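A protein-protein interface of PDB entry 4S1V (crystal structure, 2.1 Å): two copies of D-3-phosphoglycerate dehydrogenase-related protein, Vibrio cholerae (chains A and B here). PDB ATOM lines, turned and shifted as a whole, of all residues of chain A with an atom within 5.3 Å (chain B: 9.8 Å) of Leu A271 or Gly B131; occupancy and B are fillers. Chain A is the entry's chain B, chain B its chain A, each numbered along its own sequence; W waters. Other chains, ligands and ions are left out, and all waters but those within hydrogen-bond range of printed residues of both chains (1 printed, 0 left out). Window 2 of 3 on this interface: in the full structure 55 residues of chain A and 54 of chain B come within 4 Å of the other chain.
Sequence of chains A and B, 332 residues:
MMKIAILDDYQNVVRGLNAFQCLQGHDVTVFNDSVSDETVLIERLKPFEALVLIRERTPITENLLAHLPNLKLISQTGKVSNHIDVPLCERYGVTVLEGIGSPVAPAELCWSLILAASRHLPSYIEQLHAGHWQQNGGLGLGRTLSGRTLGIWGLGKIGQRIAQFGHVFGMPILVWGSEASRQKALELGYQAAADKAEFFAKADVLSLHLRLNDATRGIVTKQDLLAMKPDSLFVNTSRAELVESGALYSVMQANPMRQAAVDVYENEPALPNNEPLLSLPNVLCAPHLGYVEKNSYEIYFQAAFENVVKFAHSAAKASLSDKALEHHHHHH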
ATOM      1  N   PRO A 269      -0.819   9.589   2.870  1.00  0.00           N
ATOM      2  CA  PRO A 269      -0.588  10.306   1.609  1.00  0.00           C
ATOM      3  C   PRO A 269       0.386   9.597   0.671  1.00  0.00           C
ATOM      4  O   PRO A 269       1.402   9.078   1.122  1.00  0.00           O
ATOM      5  CB  PRO A 269       0.050  11.614   2.074  1.00  0.00           C
ATOM      6  CG  PRO A 269      -0.510  11.838   3.432  1.00  0.00           C
ATOM      7  CD  PRO A 269      -0.627  10.470   4.039  1.00  0.00           C
ATOM      8  N   ALA A 270       0.066   9.572  -0.619  1.00  0.00           N
ATOM      9  CA  ALA A 270       0.987   9.065  -1.636  1.00  0.00           C
ATOM     10  C   ALA A 270       1.717  10.252  -2.254  1.00  0.00           C
ATOM     11  O   ALA A 270       1.091  11.221  -2.668  1.00  0.00           O
ATOM     12  CB  ALA A 270       0.235   8.285  -2.697  1.00  0.00           C
ATOM     13  N   LEU A 271       3.041  10.170  -2.306  1.00  0.00           N
ATOM     14  CA  LEU A 271       3.873  11.303  -2.708  1.00  0.00           C
ATOM     15  C   LEU A 271       4.674  11.025  -3.973  1.00  0.00           C
ATOM     16  O   LEU A 271       5.058   9.881  -4.227  1.00  0.00           O
ATOM     17  CB  LEU A 271       4.824  11.690  -1.568  1.00  0.00           C
ATOM     18  CG  LEU A 271       4.226  12.310  -0.304  1.00  0.00           C
ATOM     19  CD1 LEU A 271       5.342  12.718   0.648  1.00  0.00           C
ATOM     20  CD2 LEU A 271       3.333  13.503  -0.630  1.00  0.00           C
ATOM     21  N   PRO A 272       4.937  12.076  -4.772  1.00  0.00           N
ATOM     22  CA  PRO A 272       5.789  11.936  -5.954  1.00  0.00           C
ATOM     23  C   PRO A 272       7.175  11.453  -5.572  1.00  0.00           C
ATOM     24  O   PRO A 272       7.638  11.724  -4.463  1.00  0.00           O
ATOM     25  CB  PRO A 272       5.875  13.364  -6.504  1.00  0.00           C
ATOM     26  CG  PRO A 272       4.692  14.066  -5.951  1.00  0.00           C
ATOM     27  CD  PRO A 272       4.448  13.457  -4.608  1.00  0.00           C
ATOM     28  N   ASN A 273       7.825  10.736  -6.487  1.00  0.00           N
ATOM     29  CA  ASN A 273       9.154  10.149  -6.242  1.00  0.00           C
ATOM     30  C   ASN A 273       9.200   9.076  -5.165  1.00  0.00           C
ATOM     31  O   ASN A 273      10.272   8.631  -4.739  1.00  0.00           O
ATOM     32  CB  ASN A 273      10.235  11.233  -6.135  1.00  0.00           C
ATOM     33  CG  ASN A 273      10.506  11.906  -7.466  1.00  0.00           C
ATOM     34  OD1 ASN A 273      10.708  11.238  -8.488  1.00  0.00           O
ATOM     35  ND2 ASN A 273      10.504  13.233  -7.469  1.00  0.00           N
ATOM     36  N   ASN A 274       8.006   8.664  -4.756  1.00  0.00           N
ATOM     37  CA  ASN A 274       7.793   7.645  -3.750  1.00  0.00           C
ATOM     38  C   ASN A 274       6.769   6.647  -4.295  1.00  0.00           C
ATOM     39  O   ASN A 274       7.115   5.500  -4.592  1.00  0.00           O
ATOM     40  CB  ASN A 274       7.273   8.391  -2.521  1.00  0.00           C
ATOM     41  CG  ASN A 274       7.247   7.535  -1.281  1.00  0.00           C
ATOM     42  OD1 ASN A 274       6.833   6.375  -1.311  1.00  0.00           O
ATOM     43  ND2 ASN A 274       7.690   8.110  -0.167  1.00  0.00           N
ATOM     44  N   GLU A 275       5.526   7.106  -4.456  1.00  0.00           N
ATOM     45  CA  GLU A 275       4.492   6.370  -5.180  1.00  0.00           C
ATOM     46  C   GLU A 275       4.816   6.359  -6.684  1.00  0.00           C
ATOM     47  O   GLU A 275       4.716   7.388  -7.344  1.00  0.00           O
ATOM     48  CB  GLU A 275       3.111   7.001  -4.927  1.00  0.00           C
ATOM     49  CG  GLU A 275       1.953   6.406  -5.725  1.00  0.00           C
ATOM     50  CD  GLU A 275       1.902   4.891  -5.641  1.00  0.00           C
ATOM     51  OE1 GLU A 275       1.561   4.362  -4.563  1.00  0.00           O
ATOM     52  OE2 GLU A 275       2.218   4.230  -6.649  1.00  0.00           O
ATOM     53  N   LEU A 278       2.440   7.910  -9.612  1.00  0.00           N
ATOM     54  CA  LEU A 278       2.370   9.353  -9.849  1.00  0.00           C
ATOM     55  C   LEU A 278       3.253   9.856 -10.999  1.00  0.00           C
ATOM     56  O   LEU A 278       3.174  11.023 -11.379  1.00  0.00           O
ATOM     57  CB  LEU A 278       2.688  10.120  -8.560  1.00  0.00           C
ATOM     58  CG  LEU A 278       1.529  10.190  -7.552  1.00  0.00           C
ATOM     59  CD1 LEU A 278       1.969  10.684  -6.182  1.00  0.00           C
ATOM     60  CD2 LEU A 278       0.416  11.071  -8.089  1.00  0.00           C
ATOM     61  N   SER B 123      -7.815  20.202 -10.256  1.00  0.00           N
ATOM     62  CA  SER B 123      -7.023  20.928  -9.261  1.00  0.00           C
ATOM     63  C   SER B 123      -6.439  19.984  -8.221  1.00  0.00           C
ATOM     64  O   SER B 123      -5.276  20.125  -7.830  1.00  0.00           O
ATOM     65  CB  SER B 123      -7.873  21.987  -8.562  1.00  0.00           C
ATOM     66  OG  SER B 123      -8.147  23.057  -9.440  1.00  0.00           O
ATOM     67  N   TYR B 124      -7.249  19.024  -7.775  1.00  0.00           N
ATOM     68  CA  TYR B 124      -6.786  18.013  -6.835  1.00  0.00           C
ATOM     69  C   TYR B 124      -5.659  17.171  -7.428  1.00  0.00           C
ATOM     70  O   TYR B 124      -4.712  16.817  -6.722  1.00  0.00           O
ATOM     71  CB  TYR B 124      -7.928  17.094  -6.404  1.00  0.00           C
ATOM     72  CG  TYR B 124      -8.746  17.530  -5.201  1.00  0.00           C
ATOM     73  CD1 TYR B 124      -8.172  17.630  -3.925  1.00  0.00           C
ATOM     74  CD2 TYR B 124     -10.121  17.772  -5.324  1.00  0.00           C
ATOM     75  CE1 TYR B 124      -8.937  18.003  -2.822  1.00  0.00           C
ATOM     76  CE2 TYR B 124     -10.893  18.136  -4.227  1.00  0.00           C
ATOM     77  CZ  TYR B 124     -10.302  18.241  -2.982  1.00  0.00           C
ATOM     78  OH  TYR B 124     -11.085  18.601  -1.902  1.00  0.00           O
ATOM     79  N   ILE B 125      -5.771  16.843  -8.716  1.00  0.00           N
ATOM     80  CA  ILE B 125      -4.754  16.022  -9.408  1.00  0.00           C
ATOM     81  C   ILE B 125      -3.429  16.788  -9.539  1.00  0.00           C
ATOM     82  O   ILE B 125      -2.360  16.270  -9.191  1.00  0.00           O
ATOM     83  CB  ILE B 125      -5.260  15.503 -10.783  1.00  0.00           C
ATOM     84  CG1 ILE B 125      -6.481  14.590 -10.588  1.00  0.00           C
ATOM     85  CG2 ILE B 125      -4.158  14.741 -11.536  1.00  0.00           C
ATOM     86  CD1 ILE B 125      -7.329  14.389 -11.823  1.00  0.00           C
ATOM     87  N   GLU B 126      -3.515  18.024 -10.021  1.00  0.00           N
ATOM     88  CA  GLU B 126      -2.357  18.903 -10.124  1.00  0.00           C
ATOM     89  C   GLU B 126      -1.621  19.022  -8.783  1.00  0.00           C
ATOM     90  O   GLU B 126      -0.404  18.842  -8.712  1.00  0.00           O
ATOM     91  CB  GLU B 126      -2.790  20.272 -10.653  1.00  0.00           C
ATOM     92  CG  GLU B 126      -1.687  21.321 -10.725  1.00  0.00           C
ATOM     93  CD  GLU B 126      -2.084  22.516 -11.572  1.00  0.00           C
ATOM     94  OE1 GLU B 126      -2.994  22.371 -12.423  1.00  0.00           O
ATOM     95  OE2 GLU B 126      -1.486  23.605 -11.397  1.00  0.00           O
ATOM     96  N   GLN B 127      -2.374  19.295  -7.720  1.00  0.00           N
ATOM     97  CA  GLN B 127      -1.809  19.423  -6.375  1.00  0.00           C
ATOM     98  C   GLN B 127      -1.139  18.153  -5.862  1.00  0.00           C
ATOM     99  O   GLN B 127      -0.086  18.221  -5.229  1.00  0.00           O
ATOM    100  CB  GLN B 127      -2.872  19.916  -5.387  1.00  0.00           C
ATOM    101  CG  GLN B 127      -3.187  21.393  -5.531  1.00  0.00           C
ATOM    102  CD  GLN B 127      -1.923  22.232  -5.555  1.00  0.00           C
ATOM    103  OE1 GLN B 127      -1.056  22.092  -4.694  1.00  0.00           O
ATOM    104  NE2 GLN B 127      -1.805  23.091  -6.555  1.00  0.00           N
ATOM    105  N   LEU B 128      -1.760  17.006  -6.134  1.00  0.00           N
ATOM    106  CA  LEU B 128      -1.209  15.701  -5.774  1.00  0.00           C
ATOM    107  C   LEU B 128       0.141  15.495  -6.447  1.00  0.00           C
ATOM    108  O   LEU B 128       1.098  15.058  -5.804  1.00  0.00           O
ATOM    109  CB  LEU B 128      -2.191  14.563  -6.133  1.00  0.00           C
ATOM    110  CG  LEU B 128      -1.753  13.087  -5.956  1.00  0.00           C
ATOM    111  CD1 LEU B 128      -1.269  12.795  -4.550  1.00  0.00           C
ATOM    112  CD2 LEU B 128      -2.841  12.089  -6.330  1.00  0.00           C
ATOM    113  N   HIS B 129       0.218  15.828  -7.734  1.00  0.00           N
ATOM    114  CA  HIS B 129       1.468  15.709  -8.486  1.00  0.00           C
ATOM    115  C   HIS B 129       2.550  16.661  -8.042  1.00  0.00           C
ATOM    116  O   HIS B 129       3.732  16.371  -8.226  1.00  0.00           O
ATOM    117  CB  HIS B 129       1.221  15.824  -9.984  1.00  0.00           C
ATOM    118  CG  HIS B 129       0.684  14.553 -10.611  1.00  0.00           C
ATOM    119  ND1 HIS B 129       1.460  13.478 -10.856  1.00  0.00           N
ATOM    120  CD2 HIS B 129      -0.595  14.219 -11.043  1.00  0.00           C
ATOM    121  CE1 HIS B 129       0.718  12.506 -11.420  1.00  0.00           C
ATOM    122  NE2 HIS B 129      -0.540  12.958 -11.537  1.00  0.00           N
ATOM    123  N   ALA B 130       2.170  17.794  -7.448  1.00  0.00           N
ATOM    124  CA  ALA B 130       3.161  18.717  -6.889  1.00  0.00           C
ATOM    125  C   ALA B 130       3.562  18.354  -5.445  1.00  0.00           C
ATOM    126  O   ALA B 130       4.410  19.017  -4.849  1.00  0.00           O
ATOM    127  CB  ALA B 130       2.676  20.158  -6.981  1.00  0.00           C
ATOM    128  N   GLY B 131       2.955  17.296  -4.901  1.00  0.00           N
ATOM    129  CA  GLY B 131       3.289  16.794  -3.571  1.00  0.00           C
ATOM    130  C   GLY B 131       2.456  17.350  -2.431  1.00  0.00           C
ATOM    131  O   GLY B 131       2.891  17.323  -1.280  1.00  0.00           O
ATOM    132  N   HIS B 132       1.264  17.857  -2.747  1.00  0.00           N
ATOM    133  CA  HIS B 132       0.346  18.403  -1.742  1.00  0.00           C
ATOM    134  C   HIS B 132      -0.892  17.551  -1.666  1.00  0.00           C
ATOM    135  O   HIS B 132      -1.807  17.697  -2.486  1.00  0.00           O
ATOM    136  CB  HIS B 132      -0.027  19.846  -2.069  1.00  0.00           C
ATOM    137  CG  HIS B 132       1.168  20.754  -2.296  1.00  0.00           C
ATOM    138  ND1 HIS B 132       2.175  20.859  -1.413  1.00  0.00           N
ATOM    139  CD2 HIS B 132       1.475  21.614  -3.344  1.00  0.00           C
ATOM    140  CE1 HIS B 132       3.090  21.731  -1.877  1.00  0.00           C
ATOM    141  NE2 HIS B 132       2.660  22.193  -3.056  1.00  0.00           N
ATOM    142  N   TRP B 133      -0.929  16.655  -0.681  1.00  0.00           N
ATOM    143  CA  TRP B 133      -1.976  15.641  -0.571  1.00  0.00           C
ATOM    144  C   TRP B 133      -3.340  16.188  -0.246  1.00  0.00           C
ATOM    145  O   TRP B 133      -3.551  16.789   0.815  1.00  0.00           O
ATOM    146  CB  TRP B 133      -1.571  14.594   0.455  1.00  0.00           C
ATOM    147  CG  TRP B 133      -2.631  13.545   0.671  1.00  0.00           C
ATOM    148  CD1 TRP B 133      -3.562  13.483   1.704  1.00  0.00           C
ATOM    149  CD2 TRP B 133      -2.916  12.379  -0.179  1.00  0.00           C
ATOM    150  NE1 TRP B 133      -4.373  12.391   1.562  1.00  0.00           N
ATOM    151  CE2 TRP B 133      -4.037  11.677   0.454  1.00  0.00           C
ATOM    152  CE3 TRP B 133      -2.371  11.864  -1.352  1.00  0.00           C
ATOM    153  CZ2 TRP B 133      -4.581  10.516  -0.086  1.00  0.00           C
ATOM    154  CZ3 TRP B 133      -2.923  10.686  -1.885  1.00  0.00           C
ATOM    155  CH2 TRP B 133      -4.001  10.030  -1.263  1.00  0.00           C
ATOM    156  N   GLN B 134      -4.282  15.976  -1.166  1.00  0.00           N
ATOM    157  CA  GLN B 134      -5.686  16.370  -0.989  1.00  0.00           C
ATOM    158  C   GLN B 134      -5.848  17.889  -0.829  1.00  0.00           C
ATOM    159  O   GLN B 134      -6.532  18.374   0.069  1.00  0.00           O
ATOM    160  CB  GLN B 134      -6.332  15.614   0.179  1.00  0.00           C
ATOM    161  CG  GLN B 134      -7.843  15.516   0.093  1.00  0.00           C
ATOM    162  CD  GLN B 134      -8.415  14.530   1.089  1.00  0.00           C
ATOM    163  OE1 GLN B 134      -8.847  14.910   2.176  1.00  0.00           O
ATOM    164  NE2 GLN B 134      -8.416  13.257   0.726  1.00  0.00           N
ATOM    165  N   GLN B 135      -5.201  18.623  -1.724  1.00  0.00           N
ATOM    166  CA  GLN B 135      -5.370  20.060  -1.841  1.00  0.00           C
ATOM    167  C   GLN B 135      -5.829  20.339  -3.266  1.00  0.00           C
ATOM    168  O   GLN B 135      -5.614  19.519  -4.163  1.00  0.00           O
ATOM    169  CB  GLN B 135      -4.053  20.782  -1.534  1.00  0.00           C
ATOM    170  CG  GLN B 135      -3.490  20.499  -0.147  1.00  0.00           C
ATOM    171  CD  GLN B 135      -4.311  21.136   0.964  1.00  0.00           C
ATOM    172  OE1 GLN B 135      -4.978  22.153   0.759  1.00  0.00           O
ATOM    173  NE2 GLN B 135      -4.277  20.528   2.147  1.00  0.00           N
HETATM  174  O   HOH W   1       4.048  13.902  -9.825  1.00  0.00           O
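Leu A271 touches one residue of chain B. Of the printed residues of chain A, Gly B131 touches Leu A271 (3.9 Å) and Pro A272 (3.7 Å). Ala A270 touches just these residues of chain B: Leu B128 and Trp B133. No residue of chain B comes within 4 Å of Asn A274. Printed residues of chain B within 4 Å of Pro A269: Trp B133 (3.6 Å). Printed residues of chain B within 4 Å of Leu A278: Leu B128 and His B129. Of the printed residues of chain A, His B129 touches Pro A272 (3.4 Å) and Leu A278 (2.9 Å). Printed residues of chain A within 4 Å of Trp B133: Pro A269 (3.6 Å) and Ala A270 (3.4 Å). The nearest residue of chain B that does not touch Leu A271 is Trp B133 (5.1 Å).
ND1 of His B129 lies close to O of Leu A278 (3.0 Å).
Water W1 bridges a ring nitrogen (ND1) of His B129 and the backbone carbonyl oxygen of Leu A278.
Of the 13 printed residues of chain B, 4 touch a printed residue of chain A. Hydrophobic or aromatic side chains of chain B that line the printed part of chain A: Leu B128, His B129 and Trp B133. Along chain B the printed residues that touch a printed residue of chain A span positions 128 to 133. Hydrophobic or aromatic side chains of chain A that line the printed part of chain B: Pro A269, Leu A271, Pro A272 and Leu A278. Among the printed residues, 9 pairs touch across the chains. Among the printed residues, no Asp or Glu carboxylate lies within 4 Å of a Lys or Arg side-chain nitrogen of the other chain.
No position is printed for both chains.
Among the printed residues, merely in contact across the chains: Pro A272 with His B129, Ala A270 with Leu B128, Ala A270 with Trp B133, Pro A269 with Trp B133, Leu A278 with Leu B128, Pro A272 with Gly B131, Pro A272 with Leu B128 and Leu A271 with Gly B131.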
